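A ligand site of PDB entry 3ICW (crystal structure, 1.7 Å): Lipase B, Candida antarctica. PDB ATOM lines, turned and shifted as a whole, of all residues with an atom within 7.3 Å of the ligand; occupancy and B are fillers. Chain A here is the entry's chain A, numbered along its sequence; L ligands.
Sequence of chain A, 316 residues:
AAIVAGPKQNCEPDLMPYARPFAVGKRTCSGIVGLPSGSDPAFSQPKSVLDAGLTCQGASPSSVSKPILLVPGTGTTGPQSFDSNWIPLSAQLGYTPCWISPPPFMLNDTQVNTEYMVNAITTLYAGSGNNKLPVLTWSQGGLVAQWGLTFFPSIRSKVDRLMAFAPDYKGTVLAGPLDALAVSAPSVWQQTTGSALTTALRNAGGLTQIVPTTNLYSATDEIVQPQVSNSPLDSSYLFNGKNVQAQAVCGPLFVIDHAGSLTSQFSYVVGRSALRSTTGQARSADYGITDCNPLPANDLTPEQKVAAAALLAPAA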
ATOM      1  N   PRO A  72     -10.456 -25.834  29.761  1.00  0.00           N
ATOM      2  CA  PRO A  72     -10.027 -24.490  29.333  1.00  0.00           C
ATOM      3  C   PRO A  72      -9.334 -24.322  27.982  1.00  0.00           C
ATOM      4  O   PRO A  72      -8.971 -25.295  27.326  1.00  0.00           O
ATOM      5  CB  PRO A  72      -9.130 -24.050  30.480  1.00  0.00           C
ATOM      6  CG  PRO A  72      -8.424 -25.321  30.821  1.00  0.00           C
ATOM      7  CD  PRO A  72      -9.569 -26.331  30.828  1.00  0.00           C
ATOM      8  N   GLY A  73      -9.183 -23.062  27.586  1.00  0.00           N
ATOM      9  CA  GLY A  73      -8.534 -22.732  26.327  1.00  0.00           C
ATOM     10  C   GLY A  73      -7.040 -22.538  26.491  1.00  0.00           C
ATOM     11  O   GLY A  73      -6.532 -22.478  27.617  1.00  0.00           O
ATOM     12  N   THR A  74      -6.343 -22.443  25.368  1.00  0.00           N
ATOM     13  CA  THR A  74      -4.897 -22.251  25.355  1.00  0.00           C
ATOM     14  C   THR A  74      -4.511 -20.990  26.114  1.00  0.00           C
ATOM     15  O   THR A  74      -5.156 -19.949  25.974  1.00  0.00           O
ATOM     16  CB  THR A  74      -4.380 -22.119  23.921  1.00  0.00           C
ATOM     17  OG1 THR A  74      -4.847 -23.212  23.133  1.00  0.00           O
ATOM     18  CG2 THR A  74      -2.851 -22.095  23.890  1.00  0.00           C
ATOM     19  N   GLY A  75      -3.444 -21.073  26.911  1.00  0.00           N
ATOM     20  CA  GLY A  75      -2.973 -19.932  27.672  1.00  0.00           C
ATOM     21  C   GLY A  75      -3.779 -19.573  28.905  1.00  0.00           C
ATOM     22  O   GLY A  75      -3.663 -18.460  29.408  1.00  0.00           O
ATOM     23  N   THR A  76      -4.590 -20.505  29.391  1.00  0.00           N
ATOM     24  CA  THR A  76      -5.400 -20.239  30.586  1.00  0.00           C
ATOM     25  C   THR A  76      -5.531 -21.460  31.477  1.00  0.00           C
ATOM     26  O   THR A  76      -5.188 -22.576  31.097  1.00  0.00           O
ATOM     27  CB  THR A  76      -6.852 -19.834  30.228  1.00  0.00           C
ATOM     28  OG1 THR A  76      -7.564 -20.991  29.752  1.00  0.00           O
ATOM     29  CG2 THR A  76      -6.870 -18.754  29.156  1.00  0.00           C
ATOM     30  N   SER A  81     -10.480 -19.329  32.532  1.00  0.00           N
ATOM     31  CA  SER A  81     -11.419 -19.496  31.433  1.00  0.00           C
ATOM     32  C   SER A  81     -12.881 -19.415  31.859  1.00  0.00           C
ATOM     33  O   SER A  81     -13.689 -18.786  31.183  1.00  0.00           O
ATOM     34  CB  SER A  81     -11.228 -20.868  30.758  1.00  0.00           C
ATOM     35  OG  SER A  81     -10.215 -20.861  29.768  1.00  0.00           O
ATOM     36  N   MET A 106      -2.089 -24.711  29.631  1.00  0.00           N
ATOM     37  CA  MET A 106      -2.458 -25.385  28.386  1.00  0.00           C
ATOM     38  C   MET A 106      -1.512 -25.113  27.212  1.00  0.00           C
ATOM     39  O   MET A 106      -1.866 -25.335  26.059  1.00  0.00           O
ATOM     40  CB  MET A 106      -3.890 -24.975  27.978  1.00  0.00           C
ATOM     41  CG  MET A 106      -4.998 -25.492  28.878  1.00  0.00           C
ATOM     42  SD  MET A 106      -5.380 -27.242  28.615  1.00  0.00           S
ATOM     43  CE  MET A 106      -6.373 -27.172  27.111  1.00  0.00           C
ATOM     44  N   TRP A 138     -13.822 -24.940  25.818  1.00  0.00           N
ATOM     45  CA  TRP A 138     -13.620 -23.696  25.094  1.00  0.00           C
ATOM     46  C   TRP A 138     -12.315 -23.819  24.317  1.00  0.00           C
ATOM     47  O   TRP A 138     -11.303 -24.251  24.862  1.00  0.00           O
ATOM     48  CB  TRP A 138     -13.542 -22.505  26.059  1.00  0.00           C
ATOM     49  CG  TRP A 138     -13.311 -21.183  25.369  1.00  0.00           C
ATOM     50  CD1 TRP A 138     -13.938 -20.724  24.237  1.00  0.00           C
ATOM     51  CD2 TRP A 138     -12.416 -20.139  25.773  1.00  0.00           C
ATOM     52  NE1 TRP A 138     -13.476 -19.466  23.909  1.00  0.00           N
ATOM     53  CE2 TRP A 138     -12.545 -19.087  24.839  1.00  0.00           C
ATOM     54  CE3 TRP A 138     -11.509 -19.996  26.839  1.00  0.00           C
ATOM     55  CZ2 TRP A 138     -11.805 -17.902  24.933  1.00  0.00           C
ATOM     56  CZ3 TRP A 138     -10.768 -18.820  26.929  1.00  0.00           C
ATOM     57  CH2 TRP A 138     -10.916 -17.787  25.982  1.00  0.00           C
ATOM     58  N   SER A 139     -12.371 -23.482  23.029  1.00  0.00           N
ATOM     59  CA  SER A 139     -11.194 -23.515  22.162  1.00  0.00           C
ATOM     60  C   SER A 139     -10.416 -24.843  22.174  1.00  0.00           C
ATOM     61  O   SER A 139     -10.994 -25.891  21.869  1.00  0.00           O
ATOM     62  CB  SER A 139     -10.280 -22.351  22.553  1.00  0.00           C
ATOM     63  OG  SER A 139      -9.574 -21.888  21.433  1.00  0.00           O
ATOM     64  N   GLN A 140      -9.117 -24.822  22.498  1.00  0.00           N
ATOM     65  CA  GLN A 140      -8.328 -26.063  22.520  1.00  0.00           C
ATOM     66  C   GLN A 140      -8.999 -27.139  23.386  1.00  0.00           C
ATOM     67  O   GLN A 140      -8.780 -28.331  23.171  1.00  0.00           O
ATOM     68  CB  GLN A 140      -6.902 -25.832  23.059  1.00  0.00           C
ATOM     69  CG  GLN A 140      -6.051 -27.105  22.981  1.00  0.00           C
ATOM     70  CD  GLN A 140      -4.755 -27.052  23.782  1.00  0.00           C
ATOM     71  OE1 GLN A 140      -4.101 -28.090  23.966  1.00  0.00           O
ATOM     72  NE2 GLN A 140      -4.381 -25.866  24.244  1.00  0.00           N
ATOM     73  N   GLY A 141      -9.804 -26.720  24.350  1.00  0.00           N
ATOM     74  CA  GLY A 141     -10.488 -27.679  25.201  1.00  0.00           C
ATOM     75  C   GLY A 141     -11.322 -28.673  24.402  1.00  0.00           C
ATOM     76  O   GLY A 141     -11.397 -29.849  24.764  1.00  0.00           O
ATOM     77  N   ALA A 166     -16.447 -22.650  20.396  1.00  0.00           N
ATOM     78  CA  ALA A 166     -15.326 -22.277  19.523  1.00  0.00           C
ATOM     79  C   ALA A 166     -14.209 -23.325  19.440  1.00  0.00           C
ATOM     80  O   ALA A 166     -13.019 -22.987  19.501  1.00  0.00           O
ATOM     81  CB  ALA A 166     -14.753 -20.940  19.971  1.00  0.00           C
ATOM     82  N   PRO A 167     -14.556 -24.613  19.278  1.00  0.00           N
ATOM     83  CA  PRO A 167     -13.526 -25.652  19.193  1.00  0.00           C
ATOM     84  C   PRO A 167     -12.719 -25.555  17.889  1.00  0.00           C
ATOM     85  O   PRO A 167     -13.279 -25.294  16.822  1.00  0.00           O
ATOM     86  CB  PRO A 167     -14.340 -26.947  19.258  1.00  0.00           C
ATOM     87  CG  PRO A 167     -15.605 -26.563  18.559  1.00  0.00           C
ATOM     88  CD  PRO A 167     -15.906 -25.195  19.155  1.00  0.00           C
ATOM     89  N   ASP A 168     -11.408 -25.768  17.977  1.00  0.00           N
ATOM     90  CA  ASP A 168     -10.579 -25.713  16.772  1.00  0.00           C
ATOM     91  C   ASP A 168     -10.132 -27.108  16.332  1.00  0.00           C
ATOM     92  O   ASP A 168      -8.939 -27.438  16.365  1.00  0.00           O
ATOM     93  CB  ASP A 168      -9.386 -24.774  17.003  1.00  0.00           C
ATOM     94  CG  ASP A 168      -8.486 -25.209  18.159  1.00  0.00           C
ATOM     95  OD1 ASP A 168      -8.958 -25.849  19.118  1.00  0.00           O
ATOM     96  OD2 ASP A 168      -7.278 -24.879  18.098  1.00  0.00           O
ATOM     97  N   GLY A 171      -7.763 -26.841  13.793  1.00  0.00           N
ATOM     98  CA  GLY A 171      -6.734 -25.892  14.160  1.00  0.00           C
ATOM     99  C   GLY A 171      -7.144 -24.517  13.653  1.00  0.00           C
ATOM    100  O   GLY A 171      -8.342 -24.257  13.458  1.00  0.00           O
ATOM    101  N   THR A 172      -6.179 -23.630  13.439  1.00  0.00           N
ATOM    102  CA  THR A 172      -6.491 -22.298  12.939  1.00  0.00           C
ATOM    103  C   THR A 172      -5.403 -21.849  11.962  1.00  0.00           C
ATOM    104  O   THR A 172      -4.241 -22.198  12.120  1.00  0.00           O
ATOM    105  CB  THR A 172      -6.612 -21.255  14.077  1.00  0.00           C
ATOM    106  OG1 THR A 172      -6.942 -19.979  13.526  1.00  0.00           O
ATOM    107  CG2 THR A 172      -5.302 -21.147  14.863  1.00  0.00           C
ATOM    108  N   LEU A 174      -4.788 -18.736  11.495  1.00  0.00           N
ATOM    109  CA  LEU A 174      -4.293 -17.473  12.028  1.00  0.00           C
ATOM    110  C   LEU A 174      -3.093 -17.680  12.945  1.00  0.00           C
ATOM    111  O   LEU A 174      -2.675 -16.773  13.661  1.00  0.00           O
ATOM    112  CB  LEU A 174      -5.399 -16.755  12.795  1.00  0.00           C
ATOM    113  CG  LEU A 174      -6.666 -16.444  11.989  1.00  0.00           C
ATOM    114  CD1 LEU A 174      -7.667 -15.709  12.876  1.00  0.00           C
ATOM    115  CD2 LEU A 174      -6.317 -15.593  10.772  1.00  0.00           C
ATOM    116  N   ALA A 175      -2.541 -18.889  12.932  1.00  0.00           N
ATOM    117  CA  ALA A 175      -1.382 -19.215  13.756  1.00  0.00           C
ATOM    118  C   ALA A 175      -0.109 -19.232  12.910  1.00  0.00           C
ATOM    119  O   ALA A 175       1.005 -19.220  13.448  1.00  0.00           O
ATOM    120  CB  ALA A 175      -1.574 -20.578  14.428  1.00  0.00           C
ATOM    121  N   SER A 187       1.586 -26.437  22.129  1.00  0.00           N
ATOM    122  CA  SER A 187       0.197 -26.558  21.702  1.00  0.00           C
ATOM    123  C   SER A 187      -0.181 -25.586  20.589  1.00  0.00           C
ATOM    124  O   SER A 187      -1.131 -25.822  19.848  1.00  0.00           O
ATOM    125  CB  SER A 187      -0.763 -26.370  22.891  1.00  0.00           C
ATOM    126  OG  SER A 187      -0.754 -25.037  23.362  1.00  0.00           O
ATOM    127  N   VAL A 188       0.568 -24.496  20.460  1.00  0.00           N
ATOM    128  CA  VAL A 188       0.297 -23.522  19.404  1.00  0.00           C
ATOM    129  C   VAL A 188       0.705 -24.136  18.070  1.00  0.00           C
ATOM    130  O   VAL A 188       0.009 -23.985  17.069  1.00  0.00           O
ATOM    131  CB  VAL A 188       1.053 -22.195  19.654  1.00  0.00           C
ATOM    132  CG1 VAL A 188       0.836 -21.232  18.497  1.00  0.00           C
ATOM    133  CG2 VAL A 188       0.548 -21.562  20.960  1.00  0.00           C
ATOM    134  N   TRP A 189       1.831 -24.846  18.056  1.00  0.00           N
ATOM    135  CA  TRP A 189       2.269 -25.519  16.834  1.00  0.00           C
ATOM    136  C   TRP A 189       1.214 -26.550  16.442  1.00  0.00           C
ATOM    137  O   TRP A 189       0.843 -26.680  15.276  1.00  0.00           O
ATOM    138  CB  TRP A 189       3.599 -26.257  17.048  1.00  0.00           C
ATOM    139  CG  TRP A 189       4.814 -25.405  17.021  1.00  0.00           C
ATOM    140  CD1 TRP A 189       5.392 -24.753  18.077  1.00  0.00           C
ATOM    141  CD2 TRP A 189       5.633 -25.111  15.874  1.00  0.00           C
ATOM    142  NE1 TRP A 189       6.517 -24.077  17.655  1.00  0.00           N
ATOM    143  CE2 TRP A 189       6.686 -24.278  16.309  1.00  0.00           C
ATOM    144  CE3 TRP A 189       5.570 -25.472  14.525  1.00  0.00           C
ATOM    145  CZ2 TRP A 189       7.674 -23.798  15.444  1.00  0.00           C
ATOM    146  CZ3 TRP A 189       6.545 -24.991  13.653  1.00  0.00           C
ATOM    147  CH2 TRP A 189       7.587 -24.165  14.122  1.00  0.00           C
ATOM    148  N   GLN A 191      -1.933 -26.610  17.070  1.00  0.00           N
ATOM    149  CA  GLN A 191      -3.228 -26.070  16.672  1.00  0.00           C
ATOM    150  C   GLN A 191      -3.149 -25.237  15.399  1.00  0.00           C
ATOM    151  O   GLN A 191      -4.112 -24.575  15.024  1.00  0.00           O
ATOM    152  CB  GLN A 191      -3.815 -25.231  17.796  1.00  0.00           C
ATOM    153  CG  GLN A 191      -4.096 -26.040  19.042  1.00  0.00           C
ATOM    154  CD  GLN A 191      -4.577 -25.191  20.182  1.00  0.00           C
ATOM    155  OE1 GLN A 191      -5.745 -24.829  20.256  1.00  0.00           O
ATOM    156  NE2 GLN A 191      -3.669 -24.833  21.076  1.00  0.00           N
ATOM    157  N   THR A 192      -2.001 -25.265  14.747  1.00  0.00           N
ATOM    158  CA  THR A 192      -1.824 -24.549  13.495  1.00  0.00           C
ATOM    159  C   THR A 192      -2.384 -25.452  12.409  1.00  0.00           C
ATOM    160  O   THR A 192      -2.041 -26.635  12.339  1.00  0.00           O
ATOM    161  CB  THR A 192      -0.331 -24.262  13.223  1.00  0.00           C
ATOM    162  OG1 THR A 192       0.183 -23.401  14.239  1.00  0.00           O
ATOM    163  CG2 THR A 192      -0.161 -23.606  11.859  1.00  0.00           C
ATOM    164  N   ASP A 221     -14.845 -15.027  14.704  1.00  0.00           N
ATOM    165  CA  ASP A 221     -13.844 -15.471  15.676  1.00  0.00           C
ATOM    166  C   ASP A 221     -12.497 -14.908  15.216  1.00  0.00           C
ATOM    167  O   ASP A 221     -12.074 -15.170  14.090  1.00  0.00           O
ATOM    168  CB  ASP A 221     -13.804 -17.008  15.681  1.00  0.00           C
ATOM    169  CG  ASP A 221     -13.028 -17.561  16.852  1.00  0.00           C
ATOM    170  OD1 ASP A 221     -11.891 -17.108  17.102  1.00  0.00           O
ATOM    171  OD2 ASP A 221     -13.559 -18.473  17.537  1.00  0.00           O
ATOM    172  N   GLU A 222     -11.817 -14.158  16.075  1.00  0.00           N
ATOM    173  CA  GLU A 222     -10.536 -13.556  15.698  1.00  0.00           C
ATOM    174  C   GLU A 222      -9.316 -14.437  16.012  1.00  0.00           C
ATOM    175  O   GLU A 222      -8.175 -14.055  15.746  1.00  0.00           O
ATOM    176  CB  GLU A 222     -10.361 -12.196  16.386  1.00  0.00           C
ATOM    177  CG  GLU A 222      -9.802 -12.254  17.807  1.00  0.00           C
ATOM    178  CD  GLU A 222     -10.831 -12.621  18.868  1.00  0.00           C
ATOM    179  OE1 GLU A 222     -11.913 -13.126  18.511  1.00  0.00           O
ATOM    180  OE2 GLU A 222     -10.545 -12.393  20.056  1.00  0.00           O
ATOM    181  N   ILE A 223      -9.569 -15.615  16.577  1.00  0.00           N
ATOM    182  CA  ILE A 223      -8.490 -16.543  16.917  1.00  0.00           C
ATOM    183  C   ILE A 223      -8.534 -17.806  16.069  1.00  0.00           C
ATOM    184  O   ILE A 223      -7.509 -18.277  15.578  1.00  0.00           O
ATOM    185  CB  ILE A 223      -8.564 -16.934  18.417  1.00  0.00           C
ATOM    186  CG1 ILE A 223      -8.428 -15.678  19.289  1.00  0.00           C
ATOM    187  CG2 ILE A 223      -7.499 -17.973  18.750  1.00  0.00           C
ATOM    188  CD1 ILE A 223      -7.150 -14.888  19.035  1.00  0.00           C
ATOM    189  N   VAL A 224      -9.735 -18.344  15.906  1.00  0.00           N
ATOM    190  CA  VAL A 224      -9.925 -19.562  15.124  1.00  0.00           C
ATOM    191  C   VAL A 224     -10.613 -19.309  13.790  1.00  0.00           C
ATOM    192  O   VAL A 224     -11.732 -18.793  13.744  1.00  0.00           O
ATOM    193  CB  VAL A 224     -10.792 -20.600  15.911  1.00  0.00           C
ATOM    194  CG1 VAL A 224     -10.956 -21.871  15.086  1.00  0.00           C
ATOM    195  CG2 VAL A 224     -10.152 -20.907  17.248  1.00  0.00           C
ATOM    196  N   HIS A 258     -14.013 -14.593  19.822  1.00  0.00           N
ATOM    197  CA  HIS A 258     -13.636 -15.897  20.357  1.00  0.00           C
ATOM    198  C   HIS A 258     -14.113 -16.144  21.787  1.00  0.00           C
ATOM    199  O   HIS A 258     -14.667 -17.200  22.081  1.00  0.00           O
ATOM    200  CB  HIS A 258     -12.109 -16.070  20.268  1.00  0.00           C
ATOM    201  CG  HIS A 258     -11.647 -17.443  20.623  1.00  0.00           C
ATOM    202  ND1 HIS A 258     -11.966 -18.551  19.871  1.00  0.00           N
ATOM    203  CD2 HIS A 258     -10.905 -17.896  21.664  1.00  0.00           C
ATOM    204  CE1 HIS A 258     -11.446 -19.622  20.434  1.00  0.00           C
ATOM    205  NE2 HIS A 258     -10.803 -19.257  21.530  1.00  0.00           N
HETATM  206  C1  LIG L   1      -7.168 -21.697  20.070  1.00  0.00           C
HETATM  207  C2  LIG L   1      -5.704 -21.251  20.213  1.00  0.00           C
HETATM  208  C3  LIG L   1      -4.861 -21.392  18.979  1.00  0.00           C
HETATM  209  C4  LIG L   1      -8.040 -19.523  23.918  1.00  0.00           C
HETATM  210  P1  LIG L   1      -7.910 -21.415  21.804  1.00  0.00           P
HETATM  211  O1  LIG L   1      -7.903 -19.977  22.647  1.00  0.00           O
HETATM  212  O2  LIG L   1      -7.293 -22.481  22.632  1.00  0.00           O
HETATM  213  C5  LIG L   1      -3.434 -20.922  19.222  1.00  0.00           C
HETATM  214  C6  LIG L   1      -2.943 -20.210  17.947  1.00  0.00           C
HETATM  215  C7  LIG L   1      -3.161 -18.682  18.041  1.00  0.00           C
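Merely in contact with the ligand: Gly 73, Trp 138, Asp 168, Thr 172, Ala 175, Val 188, Gln 191 and Ile 223.
Hydrophobic or aromatic side chains that line the ligand: Trp 138, Ala 175, Val 188, Ile 223 and His 258.
Within 4 Å of the ligand: Gly 73, Thr 74, Trp 138, Ser 139, Gln 140, Asp 168, Thr 172, Ala 175, Val 188, Gln 191, Ile 223 and His 258.
OG of Ser 139 is covalently linked to P1 of the ligand (1.8 Å).
N of Thr 74 sits at hydrogen-bond distance from O2 of the ligand.
OG1 of Thr 74 lies within hydrogen-bond range of O2 of the ligand (2.6 Å).
The backbone NH (N) of Gln 140 is in hydrogen-bond range of an oxygen (O2) of the ligand (3.0 Å).
O1 of the ligand is in hydrogen-bond range of NE2 of His 258.
OG of Ser 139 sits at hydrogen-bond distance from NE2 of His 258, at 2.9 Å.
The side-chain hydroxyl (OG1) of Thr 74 is in hydrogen-bond range of the side-chain amide nitrogen (NE2) of Gln 191, at 2.9 Å.
The side-chain amide nitrogen of Gln 140 sits close to the side-chain amide nitrogen of Gln 191 (3.4 Å).
A ring nitrogen (ND1) of His 258 lies within hydrogen-bond range of the side-chain carboxylate (OD2) of Asp 221 (2.8 Å).
The side-chain amide nitrogen of Gln 191 lies within hydrogen-bond range of the backbone carbonyl oxygen of Ser 187.
The backbone carbonyl oxygen of Gly 73 lies within hydrogen-bond range of the side-chain hydroxyl of Thr 76.
The side-chain hydroxyl of Ser 81 lies within hydrogen-bond range of the backbone NH of Gly 73.
The backbone carbonyl oxygen of Ile 223 sits at hydrogen-bond distance from the side-chain hydroxyl of Thr 172 (2.7 Å).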
